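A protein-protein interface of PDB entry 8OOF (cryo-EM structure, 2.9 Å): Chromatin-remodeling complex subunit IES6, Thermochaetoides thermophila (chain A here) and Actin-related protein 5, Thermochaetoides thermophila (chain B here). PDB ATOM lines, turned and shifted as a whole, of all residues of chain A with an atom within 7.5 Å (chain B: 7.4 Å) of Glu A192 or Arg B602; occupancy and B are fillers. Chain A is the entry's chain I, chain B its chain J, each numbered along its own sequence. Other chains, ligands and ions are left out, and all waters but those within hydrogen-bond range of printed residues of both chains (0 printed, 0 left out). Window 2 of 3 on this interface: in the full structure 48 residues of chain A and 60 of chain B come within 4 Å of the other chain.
The side-chain carboxylate (OE1) of Glu A192 is in salt-bridge range of the guanidinium group (NH2) of Arg B602 (3.0 Å). N of Leu B608 sits at hydrogen-bond distance from OE2 of Glu A192 (2.8 Å). The side-chain carboxylate of Glu A192 sits at hydrogen-bond distance from the backbone NH of Leu B609.
The backbone NH (N) of Glu A192 sits at hydrogen-bond distance from the side-chain amide oxygen (OD1) of Asn A190 (3.2 Å). The backbone NH (N) of Ile A193 lies within hydrogen-bond range of the side-chain amide oxygen (OD1) of Asn A190. NH2 of Arg B602 is in hydrogen-bond range of O of Lys B606 (3.1 Å). The side-chain hydroxyl (OG) of Ser B607 is in hydrogen-bond range of the backbone carbonyl oxygen (O) of Trp B604 (2.8 Å). The side-chain hydroxyl of Ser B607 lies close to the backbone NH of His B610 (3.5 Å).
His A189 touches Leu B608 (CD2 to CD2, 3.9 Å). ND2 of Asn A190 touches CD2 of Leu B608, 3.8 Å away. Glu A192 touches Ser B607 (OE2 to CB, 3.5 Å). CD2 of Leu B608 touches CD1 of Ile A193, 3.7 Å away. CD1 of Leu B609 touches CB of Met A196, 3.6 Å away.
Of the printed residues of chain B, His A189 touches Leu B608 (3.9 Å). Of the printed residues of chain B, Glu A192 touches Arg B602 (3.0 Å), Ser B607 (3.5 Å), Leu B608 (2.8 Å) and Leu B609 (3.0 Å). Printed residues of chain B within 4 Å of Ile A193: Leu B608 (3.7 Å). Arg B602 touches just one residue of chain A: Glu A192. Of the printed residues of chain A, Ser B607 touches Glu A192 (3.5 Å). His B610 touches none of the printed residues of chain A. The nearest residue of chain B that does not touch Glu A192 is Lys B606 (4.3 Å). The nearest residue of chain A that does not touch Arg B602 is Lys A191 (5.7 Å).
Of the 12 printed residues of chain A, 5 touch a printed residue of chain B. Printed residues of chain A that touch a printed residue of chain B: His A189, Asn A190, Glu A192, Ile A193 and Met A196. Hydrophobic or aromatic side chains of chain A that line the printed part of chain B: His A189, Ile A193 and Met A196. Of the 11 printed residues of chain B, 4 touch a printed residue of chain A. Among the printed residues, 8 pairs touch across the chains. Among the printed residues, Asp or Glu carboxylates within 4 Å of a Lys or Arg side-chain nitrogen of the other chain: Glu A192 with Arg B602 (3.0 Å).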
ATOM      1  N   TYR A 188      19.467 -26.015   2.453  1.00  0.00           N
ATOM      2  CA  TYR A 188      19.208 -24.864   3.301  1.00  0.00           C
ATOM      3  C   TYR A 188      18.656 -23.707   2.484  1.00  0.00           C
ATOM      4  O   TYR A 188      18.914 -23.578   1.287  1.00  0.00           O
ATOM      5  CB  TYR A 188      20.465 -24.442   4.076  1.00  0.00           C
ATOM      6  CG  TYR A 188      21.631 -24.007   3.228  1.00  0.00           C
ATOM      7  CD1 TYR A 188      22.504 -24.944   2.708  1.00  0.00           C
ATOM      8  CD2 TYR A 188      21.880 -22.668   2.978  1.00  0.00           C
ATOM      9  CE1 TYR A 188      23.571 -24.569   1.943  1.00  0.00           C
ATOM     10  CE2 TYR A 188      22.951 -22.281   2.214  1.00  0.00           C
ATOM     11  CZ  TYR A 188      23.795 -23.236   1.700  1.00  0.00           C
ATOM     12  OH  TYR A 188      24.871 -22.864   0.935  1.00  0.00           O
ATOM     13  N   HIS A 189      17.895 -22.864   3.174  1.00  0.00           N
ATOM     14  CA  HIS A 189      17.160 -21.767   2.563  1.00  0.00           C
ATOM     15  C   HIS A 189      18.052 -20.560   2.300  1.00  0.00           C
ATOM     16  O   HIS A 189      18.003 -19.969   1.217  1.00  0.00           O
ATOM     17  CB  HIS A 189      15.986 -21.384   3.465  1.00  0.00           C
ATOM     18  CG  HIS A 189      15.095 -20.328   2.896  1.00  0.00           C
ATOM     19  ND1 HIS A 189      14.382 -20.508   1.731  1.00  0.00           N
ATOM     20  CD2 HIS A 189      14.771 -19.095   3.349  1.00  0.00           C
ATOM     21  CE1 HIS A 189      13.672 -19.422   1.481  1.00  0.00           C
ATOM     22  NE2 HIS A 189      13.891 -18.550   2.449  1.00  0.00           N
ATOM     23  N   ASN A 190      18.882 -20.187   3.269  1.00  0.00           N
ATOM     24  CA  ASN A 190      19.600 -18.923   3.208  1.00  0.00           C
ATOM     25  C   ASN A 190      20.852 -19.008   4.077  1.00  0.00           C
ATOM     26  O   ASN A 190      21.143 -20.040   4.685  1.00  0.00           O
ATOM     27  CB  ASN A 190      18.671 -17.763   3.591  1.00  0.00           C
ATOM     28  CG  ASN A 190      18.258 -17.787   5.048  1.00  0.00           C
ATOM     29  OD1 ASN A 190      18.704 -18.623   5.827  1.00  0.00           O
ATOM     30  ND2 ASN A 190      17.382 -16.865   5.421  1.00  0.00           N
ATOM     31  N   LYS A 191      21.614 -17.911   4.088  1.00  0.00           N
ATOM     32  CA  LYS A 191      22.863 -17.841   4.843  1.00  0.00           C
ATOM     33  C   LYS A 191      22.658 -17.948   6.350  1.00  0.00           C
ATOM     34  O   LYS A 191      23.554 -18.416   7.058  1.00  0.00           O
ATOM     35  CB  LYS A 191      23.599 -16.543   4.505  1.00  0.00           C
ATOM     36  CG  LYS A 191      22.934 -15.291   5.044  1.00  0.00           C
ATOM     37  CD  LYS A 191      23.700 -14.045   4.660  1.00  0.00           C
ATOM     38  CE  LYS A 191      23.063 -12.819   5.278  1.00  0.00           C
ATOM     39  NZ  LYS A 191      23.803 -11.579   4.929  1.00  0.00           N
ATOM     40  N   GLU A 192      21.508 -17.509   6.863  1.00  0.00           N
ATOM     41  CA  GLU A 192      21.234 -17.657   8.290  1.00  0.00           C
ATOM     42  C   GLU A 192      21.133 -19.120   8.694  1.00  0.00           C
ATOM     43  O   GLU A 192      21.655 -19.521   9.740  1.00  0.00           O
ATOM     44  CB  GLU A 192      19.956 -16.915   8.668  1.00  0.00           C
ATOM     45  CG  GLU A 192      19.538 -17.135  10.109  1.00  0.00           C
ATOM     46  CD  GLU A 192      18.507 -16.133  10.580  1.00  0.00           C
ATOM     47  OE1 GLU A 192      18.658 -14.936  10.259  1.00  0.00           O
ATOM     48  OE2 GLU A 192      17.557 -16.533  11.285  1.00  0.00           O
ATOM     49  N   ILE A 193      20.461 -19.930   7.882  1.00  0.00           N
ATOM     50  CA  ILE A 193      20.358 -21.358   8.147  1.00  0.00           C
ATOM     51  C   ILE A 193      21.670 -22.079   7.854  1.00  0.00           C
ATOM     52  O   ILE A 193      22.001 -23.067   8.519  1.00  0.00           O
ATOM     53  CB  ILE A 193      19.174 -21.926   7.345  1.00  0.00           C
ATOM     54  CG1 ILE A 193      17.866 -21.429   7.955  1.00  0.00           C
ATOM     55  CG2 ILE A 193      19.199 -23.436   7.326  1.00  0.00           C
ATOM     56  CD1 ILE A 193      16.738 -21.330   6.981  1.00  0.00           C
ATOM     57  N   PHE A 194      22.449 -21.594   6.889  1.00  0.00           N
ATOM     58  CA  PHE A 194      23.796 -22.127   6.691  1.00  0.00           C
ATOM     59  C   PHE A 194      24.667 -21.941   7.931  1.00  0.00           C
ATOM     60  O   PHE A 194      25.458 -22.824   8.279  1.00  0.00           O
ATOM     61  CB  PHE A 194      24.447 -21.449   5.488  1.00  0.00           C
ATOM     62  CG  PHE A 194      25.756 -22.054   5.080  1.00  0.00           C
ATOM     63  CD1 PHE A 194      25.788 -23.183   4.289  1.00  0.00           C
ATOM     64  CD2 PHE A 194      26.952 -21.497   5.488  1.00  0.00           C
ATOM     65  CE1 PHE A 194      26.983 -23.740   3.904  1.00  0.00           C
ATOM     66  CE2 PHE A 194      28.151 -22.053   5.107  1.00  0.00           C
ATOM     67  CZ  PHE A 194      28.167 -23.175   4.314  1.00  0.00           C
ATOM     68  N   ALA A 195      24.550 -20.793   8.597  1.00  0.00           N
ATOM     69  CA  ALA A 195      25.265 -20.575   9.852  1.00  0.00           C
ATOM     70  C   ALA A 195      24.814 -21.548  10.937  1.00  0.00           C
ATOM     71  O   ALA A 195      25.638 -22.179  11.608  1.00  0.00           O
ATOM     72  CB  ALA A 195      25.070 -19.132  10.314  1.00  0.00           C
ATOM     73  N   MET A 196      23.500 -21.667  11.127  1.00  0.00           N
ATOM     74  CA  MET A 196      22.924 -22.657  12.035  1.00  0.00           C
ATOM     75  C   MET A 196      23.401 -24.073  11.732  1.00  0.00           C
ATOM     76  O   MET A 196      23.795 -24.815  12.637  1.00  0.00           O
ATOM     77  CB  MET A 196      21.398 -22.560  11.968  1.00  0.00           C
ATOM     78  CG  MET A 196      20.612 -23.579  12.777  1.00  0.00           C
ATOM     79  SD  MET A 196      20.347 -25.150  11.941  1.00  0.00           S
ATOM     80  CE  MET A 196      19.211 -25.929  13.072  1.00  0.00           C
ATOM     81  N   ILE A 197      23.359 -24.469  10.462  1.00  0.00           N
ATOM     82  CA  ILE A 197      23.750 -25.824  10.075  1.00  0.00           C
ATOM     83  C   ILE A 197      25.205 -26.109  10.427  1.00  0.00           C
ATOM     84  O   ILE A 197      25.530 -27.166  10.980  1.00  0.00           O
ATOM     85  CB  ILE A 197      23.478 -26.045   8.578  1.00  0.00           C
ATOM     86  CG1 ILE A 197      21.989 -26.271   8.340  1.00  0.00           C
ATOM     87  CG2 ILE A 197      24.274 -27.210   8.056  1.00  0.00           C
ATOM     88  CD1 ILE A 197      21.613 -26.250   6.887  1.00  0.00           C
ATOM     89  N   ARG A 198      26.104 -25.176  10.123  1.00  0.00           N
ATOM     90  CA  ARG A 198      27.517 -25.381  10.436  1.00  0.00           C
ATOM     91  C   ARG A 198      27.827 -25.337  11.929  1.00  0.00           C
ATOM     92  O   ARG A 198      28.851 -25.886  12.346  1.00  0.00           O
ATOM     93  CB  ARG A 198      28.363 -24.340   9.704  1.00  0.00           C
ATOM     94  CG  ARG A 198      28.426 -24.523   8.198  1.00  0.00           C
ATOM     95  CD  ARG A 198      29.134 -25.809   7.835  1.00  0.00           C
ATOM     96  NE  ARG A 198      29.282 -25.971   6.396  1.00  0.00           N
ATOM     97  CZ  ARG A 198      30.384 -25.674   5.721  1.00  0.00           C
ATOM     98  NH1 ARG A 198      31.414 -25.087   6.307  1.00  0.00           N
ATOM     99  NH2 ARG A 198      30.442 -25.943   4.421  1.00  0.00           N
ATOM    100  N   ASN A 199      26.982 -24.710  12.739  1.00  0.00           N
ATOM    101  CA  ASN A 199      27.134 -24.707  14.190  1.00  0.00           C
ATOM    102  C   ASN A 199      26.492 -25.904  14.885  1.00  0.00           C
ATOM    103  O   ASN A 199      26.574 -25.994  16.113  1.00  0.00           O
ATOM    104  CB  ASN A 199      26.560 -23.413  14.771  1.00  0.00           C
ATOM    105  CG  ASN A 199      27.333 -22.190  14.328  1.00  0.00           C
ATOM    106  OD1 ASN A 199      28.441 -22.300  13.805  1.00  0.00           O
ATOM    107  ND2 ASN A 199      26.750 -21.014  14.528  1.00  0.00           N
ATOM    108  N   GLN B 601      23.464  -4.750  14.702  1.00  0.00           N
ATOM    109  CA  GLN B 601      22.069  -4.332  14.755  1.00  0.00           C
ATOM    110  C   GLN B 601      21.146  -5.403  14.173  1.00  0.00           C
ATOM    111  O   GLN B 601      19.928  -5.229  14.117  1.00  0.00           O
ATOM    112  CB  GLN B 601      21.896  -3.002  14.017  1.00  0.00           C
ATOM    113  CG  GLN B 601      22.218  -3.066  12.531  1.00  0.00           C
ATOM    114  CD  GLN B 601      22.003  -1.739  11.829  1.00  0.00           C
ATOM    115  OE1 GLN B 601      21.646  -0.741  12.456  1.00  0.00           O
ATOM    116  NE2 GLN B 601      22.228  -1.720  10.521  1.00  0.00           N
ATOM    117  N   ARG B 602      21.745  -6.507  13.733  1.00  0.00           N
ATOM    118  CA  ARG B 602      20.997  -7.729  13.466  1.00  0.00           C
ATOM    119  C   ARG B 602      20.565  -8.364  14.785  1.00  0.00           C
ATOM    120  O   ARG B 602      21.394  -8.581  15.673  1.00  0.00           O
ATOM    121  CB  ARG B 602      21.860  -8.698  12.659  1.00  0.00           C
ATOM    122  CG  ARG B 602      21.162  -9.971  12.222  1.00  0.00           C
ATOM    123  CD  ARG B 602      20.172  -9.702  11.100  1.00  0.00           C
ATOM    124  NE  ARG B 602      19.617 -10.937  10.560  1.00  0.00           N
ATOM    125  CZ  ARG B 602      19.173 -11.081   9.319  1.00  0.00           C
ATOM    126  NH1 ARG B 602      19.190 -10.076   8.458  1.00  0.00           N
ATOM    127  NH2 ARG B 602      18.698 -12.261   8.932  1.00  0.00           N
ATOM    128  N   ASP B 603      19.274  -8.670  14.919  1.00  0.00           N
ATOM    129  CA  ASP B 603      18.772  -9.254  16.158  1.00  0.00           C
ATOM    130  C   ASP B 603      17.625 -10.217  15.868  1.00  0.00           C
ATOM    131  O   ASP B 603      17.279 -10.484  14.715  1.00  0.00           O
ATOM    132  CB  ASP B 603      18.391  -8.149  17.157  1.00  0.00           C
ATOM    133  CG  ASP B 603      17.089  -7.420  16.807  1.00  0.00           C
ATOM    134  OD1 ASP B 603      16.199  -7.970  16.127  1.00  0.00           O
ATOM    135  OD2 ASP B 603      16.956  -6.257  17.233  1.00  0.00           O
ATOM    136  N   TRP B 604      17.050 -10.751  16.954  1.00  0.00           N
ATOM    137  CA  TRP B 604      15.986 -11.751  16.872  1.00  0.00           C
ATOM    138  C   TRP B 604      14.816 -11.292  16.011  1.00  0.00           C
ATOM    139  O   TRP B 604      14.254 -12.083  15.244  1.00  0.00           O
ATOM    140  CB  TRP B 604      15.502 -12.123  18.275  1.00  0.00           C
ATOM    141  CG  TRP B 604      14.697 -11.073  18.974  1.00  0.00           C
ATOM    142  CD1 TRP B 604      15.154 -10.158  19.871  1.00  0.00           C
ATOM    143  CD2 TRP B 604      13.287 -10.855  18.861  1.00  0.00           C
ATOM    144  NE1 TRP B 604      14.120  -9.370  20.312  1.00  0.00           N
ATOM    145  CE2 TRP B 604      12.963  -9.779  19.706  1.00  0.00           C
ATOM    146  CE3 TRP B 604      12.270 -11.460  18.119  1.00  0.00           C
ATOM    147  CZ2 TRP B 604      11.666  -9.296  19.832  1.00  0.00           C
ATOM    148  CZ3 TRP B 604      10.985 -10.977  18.242  1.00  0.00           C
ATOM    149  CH2 TRP B 604      10.693  -9.907  19.093  1.00  0.00           C
ATOM    150  N   SER B 605      14.445 -10.015  16.107  1.00  0.00           N
ATOM    151  CA  SER B 605      13.285  -9.499  15.391  1.00  0.00           C
ATOM    152  C   SER B 605      13.490  -9.454  13.887  1.00  0.00           C
ATOM    153  O   SER B 605      12.548  -9.128  13.159  1.00  0.00           O
ATOM    154  CB  SER B 605      12.939  -8.103  15.906  1.00  0.00           C
ATOM    155  OG  SER B 605      11.736  -7.632  15.331  1.00  0.00           O
ATOM    156  N   LYS B 606      14.690  -9.766  13.408  1.00  0.00           N
ATOM    157  CA  LYS B 606      14.964  -9.892  11.985  1.00  0.00           C
ATOM    158  C   LYS B 606      15.604 -11.238  11.668  1.00  0.00           C
ATOM    159  O   LYS B 606      16.247 -11.386  10.625  1.00  0.00           O
ATOM    160  CB  LYS B 606      15.837  -8.737  11.491  1.00  0.00           C
ATOM    161  CG  LYS B 606      15.154  -7.387  11.641  1.00  0.00           C
ATOM    162  CD  LYS B 606      15.937  -6.270  10.992  1.00  0.00           C
ATOM    163  CE  LYS B 606      15.210  -4.944  11.148  1.00  0.00           C
ATOM    164  NZ  LYS B 606      15.948  -3.826  10.503  1.00  0.00           N
ATOM    165  N   SER B 607      15.447 -12.214  12.555  1.00  0.00           N
ATOM    166  CA  SER B 607      15.948 -13.564  12.343  1.00  0.00           C
ATOM    167  C   SER B 607      14.810 -14.502  11.961  1.00  0.00           C
ATOM    168  O   SER B 607      13.730 -14.473  12.556  1.00  0.00           O
ATOM    169  CB  SER B 607      16.665 -14.085  13.590  1.00  0.00           C
ATOM    170  OG  SER B 607      15.748 -14.377  14.624  1.00  0.00           O
ATOM    171  N   LEU B 608      15.075 -15.330  10.951  1.00  0.00           N
ATOM    172  CA  LEU B 608      14.106 -16.304  10.462  1.00  0.00           C
ATOM    173  C   LEU B 608      13.902 -17.446  11.448  1.00  0.00           C
ATOM    174  O   LEU B 608      12.772 -17.908  11.648  1.00  0.00           O
ATOM    175  CB  LEU B 608      14.572 -16.849   9.112  1.00  0.00           C
ATOM    176  CG  LEU B 608      13.744 -17.952   8.458  1.00  0.00           C
ATOM    177  CD1 LEU B 608      12.330 -17.472   8.214  1.00  0.00           C
ATOM    178  CD2 LEU B 608      14.392 -18.414   7.168  1.00  0.00           C
ATOM    179  N   LEU B 609      14.979 -17.905  12.080  1.00  0.00           N
ATOM    180  CA  LEU B 609      14.896 -19.028  13.007  1.00  0.00           C
ATOM    181  C   LEU B 609      14.149 -18.693  14.293  1.00  0.00           C
ATOM    182  O   LEU B 609      13.620 -19.601  14.940  1.00  0.00           O
ATOM    183  CB  LEU B 609      16.296 -19.538  13.326  1.00  0.00           C
ATOM    184  CG  LEU B 609      16.968 -20.277  12.172  1.00  0.00           C
ATOM    185  CD1 LEU B 609      18.423 -20.534  12.486  1.00  0.00           C
ATOM    186  CD2 LEU B 609      16.245 -21.578  11.887  1.00  0.00           C
ATOM    187  N   HIS B 610      14.087 -17.425  14.693  1.00  0.00           N
ATOM    188  CA  HIS B 610      13.174 -17.071  15.776  1.00  0.00           C
ATOM    189  C   HIS B 610      11.718 -17.188  15.347  1.00  0.00           C
ATOM    190  O   HIS B 610      10.887 -17.723  16.088  1.00  0.00           O
ATOM    191  CB  HIS B 610      13.465 -15.658  16.275  1.00  0.00           C
ATOM    192  CG  HIS B 610      12.618 -15.244  17.436  1.00  0.00           C
ATOM    193  ND1 HIS B 610      13.040 -15.344  18.743  1.00  0.00           N
ATOM    194  CD2 HIS B 610      11.370 -14.722  17.483  1.00  0.00           C
ATOM    195  CE1 HIS B 610      12.088 -14.904  19.545  1.00  0.00           C
ATOM    196  NE2 HIS B 610      11.063 -14.523  18.806  1.00  0.00           N
ATOM    197  N   ALA B 611      11.379 -16.667  14.168  1.00  0.00           N
ATOM    198  CA  ALA B 611      10.020 -16.810  13.656  1.00  0.00           C
ATOM    199  C   ALA B 611       9.617 -18.275  13.558  1.00  0.00           C
ATOM    200  O   ALA B 611       8.539 -18.671  14.011  1.00  0.00           O
ATOM    201  CB  ALA B 611       9.902 -16.127  12.294  1.00  0.00           C
